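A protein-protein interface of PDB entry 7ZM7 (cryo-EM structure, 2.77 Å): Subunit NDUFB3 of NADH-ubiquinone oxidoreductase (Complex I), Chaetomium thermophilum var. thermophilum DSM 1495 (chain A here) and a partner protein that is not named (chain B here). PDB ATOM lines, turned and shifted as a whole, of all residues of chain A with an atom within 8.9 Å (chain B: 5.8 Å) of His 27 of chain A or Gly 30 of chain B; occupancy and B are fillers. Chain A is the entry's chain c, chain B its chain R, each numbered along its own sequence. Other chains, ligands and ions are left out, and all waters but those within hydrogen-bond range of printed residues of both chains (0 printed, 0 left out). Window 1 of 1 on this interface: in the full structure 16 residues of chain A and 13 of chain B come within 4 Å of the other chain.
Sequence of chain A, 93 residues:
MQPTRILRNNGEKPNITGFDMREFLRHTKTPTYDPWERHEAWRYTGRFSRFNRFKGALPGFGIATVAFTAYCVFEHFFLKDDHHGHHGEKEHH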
ATOM      1  N   ASP A  20     -21.651 -23.053 -31.324  1.00  0.00           N
ATOM      2  CA  ASP A  20     -21.439 -24.482 -31.168  1.00  0.00           C
ATOM      3  C   ASP A  20     -21.778 -24.837 -29.730  1.00  0.00           C
ATOM      4  O   ASP A  20     -21.549 -24.038 -28.820  1.00  0.00           O
ATOM      5  CB  ASP A  20     -19.988 -24.868 -31.517  1.00  0.00           C
ATOM      6  CG  ASP A  20     -19.678 -26.346 -31.282  1.00  0.00           C
ATOM      7  OD1 ASP A  20     -20.125 -26.936 -30.278  1.00  0.00           O
ATOM      8  OD2 ASP A  20     -18.964 -26.929 -32.126  1.00  0.00           O
ATOM      9  N   MET A  21     -22.326 -26.037 -29.528  1.00  0.00           N
ATOM     10  CA  MET A  21     -22.708 -26.450 -28.182  1.00  0.00           C
ATOM     11  C   MET A  21     -21.495 -26.630 -27.282  1.00  0.00           C
ATOM     12  O   MET A  21     -21.528 -26.247 -26.106  1.00  0.00           O
ATOM     13  CB  MET A  21     -23.521 -27.740 -28.231  1.00  0.00           C
ATOM     14  CG  MET A  21     -24.864 -27.601 -28.907  1.00  0.00           C
ATOM     15  SD  MET A  21     -25.898 -26.408 -28.040  1.00  0.00           S
ATOM     16  CE  MET A  21     -26.238 -27.273 -26.515  1.00  0.00           C
ATOM     17  N   ARG A  22     -20.420 -27.219 -27.806  1.00  0.00           N
ATOM     18  CA  ARG A  22     -19.276 -27.545 -26.960  1.00  0.00           C
ATOM     19  C   ARG A  22     -18.675 -26.289 -26.345  1.00  0.00           C
ATOM     20  O   ARG A  22     -18.366 -26.255 -25.149  1.00  0.00           O
ATOM     21  CB  ARG A  22     -18.229 -28.309 -27.768  1.00  0.00           C
ATOM     22  CG  ARG A  22     -18.503 -29.800 -27.882  1.00  0.00           C
ATOM     23  CD  ARG A  22     -18.281 -30.508 -26.557  1.00  0.00           C
ATOM     24  NE  ARG A  22     -19.216 -31.614 -26.372  1.00  0.00           N
ATOM     25  CZ  ARG A  22     -19.520 -32.147 -25.193  1.00  0.00           C
ATOM     26  NH1 ARG A  22     -18.959 -31.677 -24.086  1.00  0.00           N
ATOM     27  NH2 ARG A  22     -20.383 -33.151 -25.119  1.00  0.00           N
ATOM     28  N   GLU A  23     -18.514 -25.236 -27.146  1.00  0.00           N
ATOM     29  CA  GLU A  23     -18.021 -23.976 -26.603  1.00  0.00           C
ATOM     30  C   GLU A  23     -19.078 -23.308 -25.736  1.00  0.00           C
ATOM     31  O   GLU A  23     -18.752 -22.620 -24.763  1.00  0.00           O
ATOM     32  CB  GLU A  23     -17.584 -23.052 -27.738  1.00  0.00           C
ATOM     33  CG  GLU A  23     -16.386 -23.572 -28.507  1.00  0.00           C
ATOM     34  CD  GLU A  23     -15.127 -23.605 -27.667  1.00  0.00           C
ATOM     35  OE1 GLU A  23     -14.980 -22.744 -26.775  1.00  0.00           O
ATOM     36  OE2 GLU A  23     -14.287 -24.502 -27.891  1.00  0.00           O
ATOM     37  N   PHE A  24     -20.352 -23.499 -26.078  1.00  0.00           N
ATOM     38  CA  PHE A  24     -21.432 -22.956 -25.263  1.00  0.00           C
ATOM     39  C   PHE A  24     -21.405 -23.537 -23.859  1.00  0.00           C
ATOM     40  O   PHE A  24     -21.540 -22.806 -22.872  1.00  0.00           O
ATOM     41  CB  PHE A  24     -22.774 -23.247 -25.928  1.00  0.00           C
ATOM     42  CG  PHE A  24     -23.940 -22.579 -25.270  1.00  0.00           C
ATOM     43  CD1 PHE A  24     -24.031 -21.206 -25.220  1.00  0.00           C
ATOM     44  CD2 PHE A  24     -24.956 -23.329 -24.714  1.00  0.00           C
ATOM     45  CE1 PHE A  24     -25.110 -20.600 -24.623  1.00  0.00           C
ATOM     46  CE2 PHE A  24     -26.032 -22.726 -24.121  1.00  0.00           C
ATOM     47  CZ  PHE A  24     -26.110 -21.367 -24.075  1.00  0.00           C
ATOM     48  N   LEU A  25     -21.218 -24.851 -23.749  1.00  0.00           N
ATOM     49  CA  LEU A  25     -21.210 -25.496 -22.447  1.00  0.00           C
ATOM     50  C   LEU A  25     -19.950 -25.180 -21.658  1.00  0.00           C
ATOM     51  O   LEU A  25     -20.008 -25.076 -20.430  1.00  0.00           O
ATOM     52  CB  LEU A  25     -21.349 -27.006 -22.618  1.00  0.00           C
ATOM     53  CG  LEU A  25     -22.722 -27.523 -23.037  1.00  0.00           C
ATOM     54  CD1 LEU A  25     -22.709 -29.036 -23.097  1.00  0.00           C
ATOM     55  CD2 LEU A  25     -23.795 -27.033 -22.081  1.00  0.00           C
ATOM     56  N   ARG A  26     -18.809 -25.038 -22.334  1.00  0.00           N
ATOM     57  CA  ARG A  26     -17.567 -24.763 -21.623  1.00  0.00           C
ATOM     58  C   ARG A  26     -17.593 -23.395 -20.965  1.00  0.00           C
ATOM     59  O   ARG A  26     -17.011 -23.214 -19.892  1.00  0.00           O
ATOM     60  CB  ARG A  26     -16.377 -24.871 -22.577  1.00  0.00           C
ATOM     61  N   HIS A  27     -18.257 -22.426 -21.585  1.00  0.00           N
ATOM     62  CA  HIS A  27     -18.350 -21.089 -21.018  1.00  0.00           C
ATOM     63  C   HIS A  27     -19.339 -21.011 -19.868  1.00  0.00           C
ATOM     64  O   HIS A  27     -19.441 -19.958 -19.231  1.00  0.00           O
ATOM     65  CB  HIS A  27     -18.747 -20.085 -22.100  1.00  0.00           C
ATOM     66  CG  HIS A  27     -17.587 -19.537 -22.868  1.00  0.00           C
ATOM     67  ND1 HIS A  27     -17.674 -18.392 -23.628  1.00  0.00           N
ATOM     68  CD2 HIS A  27     -16.313 -19.977 -22.993  1.00  0.00           C
ATOM     69  CE1 HIS A  27     -16.504 -18.150 -24.190  1.00  0.00           C
ATOM     70  NE2 HIS A  27     -15.661 -19.096 -23.820  1.00  0.00           N
ATOM     71  N   THR A  28     -20.063 -22.092 -19.587  1.00  0.00           N
ATOM     72  CA  THR A  28     -21.033 -22.105 -18.504  1.00  0.00           C
ATOM     73  C   THR A  28     -20.336 -22.154 -17.159  1.00  0.00           C
ATOM     74  O   THR A  28     -20.399 -23.164 -16.455  1.00  0.00           O
ATOM     75  CB  THR A  28     -21.976 -23.292 -18.644  1.00  0.00           C
ATOM     76  OG1 THR A  28     -21.224 -24.510 -18.576  1.00  0.00           O
ATOM     77  CG2 THR A  28     -22.720 -23.221 -19.960  1.00  0.00           C
ATOM     78  N   LYS A  29     -19.681 -21.059 -16.792  1.00  0.00           N
ATOM     79  CA  LYS A  29     -19.005 -20.946 -15.512  1.00  0.00           C
ATOM     80  C   LYS A  29     -18.964 -19.474 -15.145  1.00  0.00           C
ATOM     81  O   LYS A  29     -19.314 -18.608 -15.949  1.00  0.00           O
ATOM     82  CB  LYS A  29     -17.597 -21.545 -15.560  1.00  0.00           C
ATOM     83  N   THR A  30     -18.544 -19.195 -13.922  1.00  0.00           N
ATOM     84  CA  THR A  30     -18.502 -17.815 -13.469  1.00  0.00           C
ATOM     85  C   THR A  30     -17.491 -17.046 -14.308  1.00  0.00           C
ATOM     86  O   THR A  30     -16.312 -17.427 -14.345  1.00  0.00           O
ATOM     87  CB  THR A  30     -18.133 -17.739 -11.994  1.00  0.00           C
ATOM     88  OG1 THR A  30     -19.223 -18.227 -11.204  1.00  0.00           O
ATOM     89  CG2 THR A  30     -17.841 -16.304 -11.600  1.00  0.00           C
ATOM     90  N   PRO A  31     -17.899 -15.989 -15.000  1.00  0.00           N
ATOM     91  CA  PRO A  31     -16.953 -15.258 -15.845  1.00  0.00           C
ATOM     92  C   PRO A  31     -15.906 -14.541 -15.012  1.00  0.00           C
ATOM     93  O   PRO A  31     -16.166 -14.087 -13.896  1.00  0.00           O
ATOM     94  CB  PRO A  31     -17.844 -14.261 -16.592  1.00  0.00           C
ATOM     95  CG  PRO A  31     -19.031 -14.090 -15.713  1.00  0.00           C
ATOM     96  CD  PRO A  31     -19.249 -15.409 -15.042  1.00  0.00           C
ATOM     97  N   THR A  32     -14.701 -14.450 -15.572  1.00  0.00           N
ATOM     98  CA  THR A  32     -13.637 -13.720 -14.895  1.00  0.00           C
ATOM     99  C   THR A  32     -13.910 -12.223 -14.900  1.00  0.00           C
ATOM    100  O   THR A  32     -13.710 -11.544 -13.886  1.00  0.00           O
ATOM    101  CB  THR A  32     -12.294 -14.020 -15.555  1.00  0.00           C
ATOM    102  OG1 THR A  32     -12.330 -13.591 -16.921  1.00  0.00           O
ATOM    103  CG2 THR A  32     -12.002 -15.511 -15.506  1.00  0.00           C
ATOM    104  N   TYR A  33     -14.372 -11.693 -16.028  1.00  0.00           N
ATOM    105  CA  TYR A  33     -14.692 -10.282 -16.174  1.00  0.00           C
ATOM    106  C   TYR A  33     -16.109 -10.135 -16.707  1.00  0.00           C
ATOM    107  O   TYR A  33     -16.510 -10.849 -17.629  1.00  0.00           O
ATOM    108  CB  TYR A  33     -13.706  -9.592 -17.113  1.00  0.00           C
ATOM    109  CG  TYR A  33     -14.216  -8.288 -17.668  1.00  0.00           C
ATOM    110  CD1 TYR A  33     -14.409  -7.192 -16.844  1.00  0.00           C
ATOM    111  CD2 TYR A  33     -14.502  -8.153 -19.017  1.00  0.00           C
ATOM    112  CE1 TYR A  33     -14.875  -5.999 -17.346  1.00  0.00           C
ATOM    113  CE2 TYR A  33     -14.966  -6.965 -19.529  1.00  0.00           C
ATOM    114  CZ  TYR A  33     -15.151  -5.890 -18.689  1.00  0.00           C
ATOM    115  OH  TYR A  33     -15.615  -4.700 -19.195  1.00  0.00           O
ATOM    116  N   ASP A  34     -16.860  -9.203 -16.130  1.00  0.00           N
ATOM    117  CA  ASP A  34     -18.258  -9.032 -16.496  1.00  0.00           C
ATOM    118  C   ASP A  34     -18.631  -7.558 -16.535  1.00  0.00           C
ATOM    119  O   ASP A  34     -18.451  -6.849 -15.538  1.00  0.00           O
ATOM    120  CB  ASP A  34     -19.160  -9.765 -15.505  1.00  0.00           C
ATOM    121  CG  ASP A  34     -20.615  -9.745 -15.916  1.00  0.00           C
ATOM    122  OD1 ASP A  34     -20.900  -9.566 -17.118  1.00  0.00           O
ATOM    123  OD2 ASP A  34     -21.479  -9.884 -15.027  1.00  0.00           O
ATOM    124  N   PRO A  35     -19.154  -7.064 -17.656  1.00  0.00           N
ATOM    125  CA  PRO A  35     -19.614  -5.669 -17.697  1.00  0.00           C
ATOM    126  C   PRO A  35     -20.736  -5.380 -16.724  1.00  0.00           C
ATOM    127  O   PRO A  35     -20.962  -4.215 -16.391  1.00  0.00           O
ATOM    128  CB  PRO A  35     -20.081  -5.499 -19.145  1.00  0.00           C
ATOM    129  CG  PRO A  35     -19.375  -6.560 -19.901  1.00  0.00           C
ATOM    130  CD  PRO A  35     -19.237  -7.713 -18.971  1.00  0.00           C
ATOM    131  N   GLU A  37     -20.803  -6.862 -13.661  1.00  0.00           N
ATOM    132  CA  GLU A  37     -20.339  -7.504 -12.436  1.00  0.00           C
ATOM    133  C   GLU A  37     -20.865  -6.791 -11.198  1.00  0.00           C
ATOM    134  O   GLU A  37     -21.369  -7.431 -10.270  1.00  0.00           O
ATOM    135  CB  GLU A  37     -18.812  -7.553 -12.422  1.00  0.00           C
ATOM    136  CG  GLU A  37     -18.225  -8.242 -11.201  1.00  0.00           C
ATOM    137  CD  GLU A  37     -18.571  -9.714 -11.132  1.00  0.00           C
ATOM    138  OE1 GLU A  37     -18.822 -10.320 -12.194  1.00  0.00           O
ATOM    139  OE2 GLU A  37     -18.593 -10.270 -10.014  1.00  0.00           O
ATOM    140  N   GLU A  40     -24.806  -7.128 -10.620  1.00  0.00           N
ATOM    141  CA  GLU A  40     -25.272  -8.407 -10.104  1.00  0.00           C
ATOM    142  C   GLU A  40     -24.534  -8.828  -8.843  1.00  0.00           C
ATOM    143  O   GLU A  40     -24.752  -9.933  -8.341  1.00  0.00           O
ATOM    144  CB  GLU A  40     -25.146  -9.488 -11.177  1.00  0.00           C
ATOM    145  CG  GLU A  40     -26.074  -9.288 -12.353  1.00  0.00           C
ATOM    146  CD  GLU A  40     -25.912 -10.362 -13.404  1.00  0.00           C
ATOM    147  OE1 GLU A  40     -24.988 -11.189 -13.268  1.00  0.00           O
ATOM    148  OE2 GLU A  40     -26.712 -10.380 -14.361  1.00  0.00           O
ATOM    149  N   TYR A  44     -24.960 -12.625  -4.594  1.00  0.00           N
ATOM    150  CA  TYR A  44     -24.056 -13.693  -4.086  1.00  0.00           C
ATOM    151  C   TYR A  44     -23.271 -13.229  -2.859  1.00  0.00           C
ATOM    152  O   TYR A  44     -22.393 -13.989  -2.412  1.00  0.00           O
ATOM    153  CB  TYR A  44     -23.135 -14.177  -5.208  1.00  0.00           C
ATOM    154  CG  TYR A  44     -23.740 -14.082  -6.586  1.00  0.00           C
ATOM    155  CD1 TYR A  44     -24.699 -14.985  -7.011  1.00  0.00           C
ATOM    156  CD2 TYR A  44     -23.365 -13.078  -7.462  1.00  0.00           C
ATOM    157  CE1 TYR A  44     -25.270 -14.896  -8.268  1.00  0.00           C
ATOM    158  CE2 TYR A  44     -23.921 -12.978  -8.726  1.00  0.00           C
ATOM    159  CZ  TYR A  44     -24.879 -13.888  -9.131  1.00  0.00           C
ATOM    160  OH  TYR A  44     -25.430 -13.792 -10.375  1.00  0.00           O
ATOM    161  N   ARG B  25     -28.336 -17.482 -12.064  1.00  0.00           N
ATOM    162  CA  ARG B  25     -28.046 -16.279 -12.836  1.00  0.00           C
ATOM    163  C   ARG B  25     -26.557 -16.114 -13.091  1.00  0.00           C
ATOM    164  O   ARG B  25     -26.161 -15.641 -14.160  1.00  0.00           O
ATOM    165  CB  ARG B  25     -28.604 -15.048 -12.128  1.00  0.00           C
ATOM    166  CG  ARG B  25     -30.068 -14.802 -12.409  1.00  0.00           C
ATOM    167  CD  ARG B  25     -30.553 -13.550 -11.705  1.00  0.00           C
ATOM    168  NE  ARG B  25     -30.020 -12.326 -12.301  1.00  0.00           N
ATOM    169  CZ  ARG B  25     -30.268 -11.908 -13.540  1.00  0.00           C
ATOM    170  NH1 ARG B  25     -31.064 -12.601 -14.344  1.00  0.00           N
ATOM    171  NH2 ARG B  25     -29.727 -10.780 -13.972  1.00  0.00           N
ATOM    172  N   ASN B  26     -25.717 -16.486 -12.122  1.00  0.00           N
ATOM    173  CA  ASN B  26     -24.279 -16.304 -12.296  1.00  0.00           C
ATOM    174  C   ASN B  26     -23.773 -17.070 -13.507  1.00  0.00           C
ATOM    175  O   ASN B  26     -23.020 -16.529 -14.323  1.00  0.00           O
ATOM    176  CB  ASN B  26     -23.530 -16.753 -11.044  1.00  0.00           C
ATOM    177  CG  ASN B  26     -23.988 -18.101 -10.550  1.00  0.00           C
ATOM    178  OD1 ASN B  26     -24.922 -18.684 -11.093  1.00  0.00           O
ATOM    179  ND2 ASN B  26     -23.327 -18.610  -9.519  1.00  0.00           N
ATOM    180  N   LEU B  27     -24.189 -18.324 -13.649  1.00  0.00           N
ATOM    181  CA  LEU B  27     -23.703 -19.139 -14.753  1.00  0.00           C
ATOM    182  C   LEU B  27     -24.219 -18.620 -16.092  1.00  0.00           C
ATOM    183  O   LEU B  27     -23.484 -18.597 -17.084  1.00  0.00           O
ATOM    184  CB  LEU B  27     -24.101 -20.592 -14.520  1.00  0.00           C
ATOM    185  CG  LEU B  27     -23.523 -21.635 -15.465  1.00  0.00           C
ATOM    186  CD1 LEU B  27     -23.395 -22.960 -14.731  1.00  0.00           C
ATOM    187  CD2 LEU B  27     -24.387 -21.787 -16.699  1.00  0.00           C
ATOM    188  N   TRP B  28     -25.480 -18.195 -16.134  1.00  0.00           N
ATOM    189  CA  TRP B  28     -26.042 -17.651 -17.361  1.00  0.00           C
ATOM    190  C   TRP B  28     -25.357 -16.362 -17.767  1.00  0.00           C
ATOM    191  O   TRP B  28     -25.277 -16.054 -18.959  1.00  0.00           O
ATOM    192  CB  TRP B  28     -27.531 -17.404 -17.186  1.00  0.00           C
ATOM    193  CG  TRP B  28     -28.129 -16.538 -18.224  1.00  0.00           C
ATOM    194  CD1 TRP B  28     -28.598 -16.925 -19.429  1.00  0.00           C
ATOM    195  CD2 TRP B  28     -28.330 -15.130 -18.145  1.00  0.00           C
ATOM    196  NE1 TRP B  28     -29.090 -15.851 -20.115  1.00  0.00           N
ATOM    197  CE2 TRP B  28     -28.937 -14.731 -19.345  1.00  0.00           C
ATOM    198  CE3 TRP B  28     -28.064 -14.170 -17.174  1.00  0.00           C
ATOM    199  CZ2 TRP B  28     -29.276 -13.417 -19.601  1.00  0.00           C
ATOM    200  CZ3 TRP B  28     -28.407 -12.873 -17.428  1.00  0.00           C
ATOM    201  CH2 TRP B  28     -29.004 -12.505 -18.631  1.00  0.00           C
ATOM    202  N   ARG B  29     -24.876 -15.591 -16.797  1.00  0.00           N
ATOM    203  CA  ARG B  29     -24.155 -14.369 -17.115  1.00  0.00           C
ATOM    204  C   ARG B  29     -22.931 -14.674 -17.967  1.00  0.00           C
ATOM    205  O   ARG B  29     -22.733 -14.075 -19.028  1.00  0.00           O
ATOM    206  CB  ARG B  29     -23.763 -13.666 -15.823  1.00  0.00           C
ATOM    207  CG  ARG B  29     -23.360 -12.245 -15.995  1.00  0.00           C
ATOM    208  CD  ARG B  29     -24.507 -11.435 -16.524  1.00  0.00           C
ATOM    209  NE  ARG B  29     -24.238 -10.927 -17.858  1.00  0.00           N
ATOM    210  CZ  ARG B  29     -25.168 -10.435 -18.665  1.00  0.00           C
ATOM    211  NH1 ARG B  29     -26.433 -10.398 -18.272  1.00  0.00           N
ATOM    212  NH2 ARG B  29     -24.836  -9.985 -19.865  1.00  0.00           N
ATOM    213  N   GLY B  30     -22.107 -15.622 -17.527  1.00  0.00           N
ATOM    214  CA  GLY B  30     -21.020 -16.073 -18.375  1.00  0.00           C
ATOM    215  C   GLY B  30     -21.535 -16.706 -19.648  1.00  0.00           C
ATOM    216  O   GLY B  30     -20.971 -16.507 -20.726  1.00  0.00           O
ATOM    217  N   GLN B  31     -22.616 -17.470 -19.541  1.00  0.00           N
ATOM    218  CA  GLN B  31     -23.263 -18.027 -20.719  1.00  0.00           C
ATOM    219  C   GLN B  31     -23.803 -16.928 -21.625  1.00  0.00           C
ATOM    220  O   GLN B  31     -23.878 -17.107 -22.843  1.00  0.00           O
ATOM    221  CB  GLN B  31     -24.381 -18.962 -20.271  1.00  0.00           C
ATOM    222  CG  GLN B  31     -24.696 -20.100 -21.197  1.00  0.00           C
ATOM    223  CD  GLN B  31     -25.887 -20.895 -20.717  1.00  0.00           C
ATOM    224  OE1 GLN B  31     -26.860 -20.334 -20.215  1.00  0.00           O
ATOM    225  NE2 GLN B  31     -25.812 -22.209 -20.850  1.00  0.00           N
ATOM    226  N   ALA B  32     -24.173 -15.787 -21.049  1.00  0.00           N
ATOM    227  CA  ALA B  32     -24.738 -14.700 -21.842  1.00  0.00           C
ATOM    228  C   ALA B  32     -23.680 -14.030 -22.708  1.00  0.00           C
ATOM    229  O   ALA B  32     -23.892 -13.809 -23.904  1.00  0.00           O
ATOM    230  CB  ALA B  32     -25.400 -13.678 -20.921  1.00  0.00           C
ATOM    231  N   LEU B  33     -22.532 -13.696 -22.118  1.00  0.00           N
ATOM    232  CA  LEU B  33     -21.523 -12.931 -22.840  1.00  0.00           C
ATOM    233  C   LEU B  33     -21.013 -13.673 -24.066  1.00  0.00           C
ATOM    234  O   LEU B  33     -20.557 -13.041 -25.024  1.00  0.00           O
ATOM    235  CB  LEU B  33     -20.373 -12.571 -21.899  1.00  0.00           C
ATOM    236  CG  LEU B  33     -19.551 -13.678 -21.237  1.00  0.00           C
ATOM    237  CD1 LEU B  33     -18.446 -14.212 -22.136  1.00  0.00           C
ATOM    238  CD2 LEU B  33     -18.967 -13.154 -19.938  1.00  0.00           C
ATOM    239  N   TYR B  34     -21.077 -15.005 -24.054  1.00  0.00           N
ATOM    240  CA  TYR B  34     -20.750 -15.768 -25.249  1.00  0.00           C
ATOM    241  C   TYR B  34     -21.687 -15.421 -26.397  1.00  0.00           C
ATOM    242  O   TYR B  34     -21.241 -15.278 -27.539  1.00  0.00           O
ATOM    243  CB  TYR B  34     -20.804 -17.260 -24.938  1.00  0.00           C
ATOM    244  CG  TYR B  34     -20.442 -18.158 -26.096  1.00  0.00           C
ATOM    245  CD1 TYR B  34     -19.125 -18.321 -26.486  1.00  0.00           C
ATOM    246  CD2 TYR B  34     -21.418 -18.850 -26.789  1.00  0.00           C
ATOM    247  CE1 TYR B  34     -18.792 -19.146 -27.538  1.00  0.00           C
ATOM    248  CE2 TYR B  34     -21.095 -19.678 -27.839  1.00  0.00           C
ATOM    249  CZ  TYR B  34     -19.782 -19.820 -28.211  1.00  0.00           C
ATOM    250  OH  TYR B  34     -19.457 -20.643 -29.262  1.00  0.00           O
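The backbone NH of Asn 26 of chain B is in hydrogen-bond range of the side-chain hydroxyl of Tyr 44 of chain A (3.2 Å). The side-chain carboxylate of Asp 34 of chain A lies within salt-bridge range of the guanidinium group of Arg 29 of chain B (3.7 Å). NH2 of Arg 25 of chain B is in salt-bridge range of OE2 of Glu 40 of chain A, 3.1 Å away. NH1 of Arg 29 of chain B lies within salt-bridge range of OE2 of Glu 40 of chain A, at 3.9 Å.
The side-chain carboxylate (OD1) of Asp 20 of chain A lies within hydrogen-bond range of the backbone NH (N) of Arg 22 of chain A (2.5 Å). OD2 of Asp 34 of chain A sits at hydrogen-bond distance from N of Glu 37 of chain A, 3.4 Å away.
Among the printed residues, merely in contact across the chains: His 27 of chain A with Tyr 34 of chain B, Phe 24 of chain A with Gln 31 of chain B, Thr 28 of chain A with Gln 31 of chain B, Glu 23 of chain A with Tyr 34 of chain B, Thr 28 of chain A with Leu 27 of chain B, Pro 31 of chain A with Leu 33 of chain B, Tyr 44 of chain A with Arg 25 of chain B, Pro 31 of chain A with Gly 30 of chain B, Phe 24 of chain A with Tyr 34 of chain B, Asp 20 of chain A with Tyr 34 of chain B, His 27 of chain A with Gly 30 of chain B, Lys 29 of chain A with Gly 30 of chain B and Pro 31 of chain A with Asn 26 of chain B.
Printed residues of chain B within 4 Å of Lys 29 of chain A: Gly 30. Thr 32 of chain A touches none of the printed residues of chain B. Of the printed residues of chain B, Asp 34 of chain A touches Arg 29. Pro 35 of chain A touches none of the printed residues of chain B. Printed residues of chain B within 4 Å of Tyr 44 of chain A: Arg 25 (3.7 Å) and Asn 26 (3.2 Å). Of the printed residues of chain A, Leu 27 of chain B touches Thr 28 (3.4 Å). Gly 30 of chain B touches just these residues of chain A: His 27, Lys 29 and Pro 31. The nearest residue of chain B that does not touch His 27 of chain A is Gln 31 of chain B (4.05 Å).
Of the 19 printed residues of chain A, 10 touch a printed residue of chain B. Hydrophobic or aromatic side chains of chain A within 4 Å of the printed part of chain B: Phe 24, His 27, Pro 31 and Tyr 44. Along chain B the printed residues that touch a printed residue of chain A span positions 25 to 34. Among the printed residues, Asp or Glu carboxylates within 4 Å of a Lys or Arg side-chain nitrogen of the other chain: Asp 34 of chain A with Arg 29 of chain B (3.7 Å), Glu 40 of chain A with Arg 25 of chain B (3.1 Å) and Glu 40 of chain A with Arg 29 of chain B (3.9 Å).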
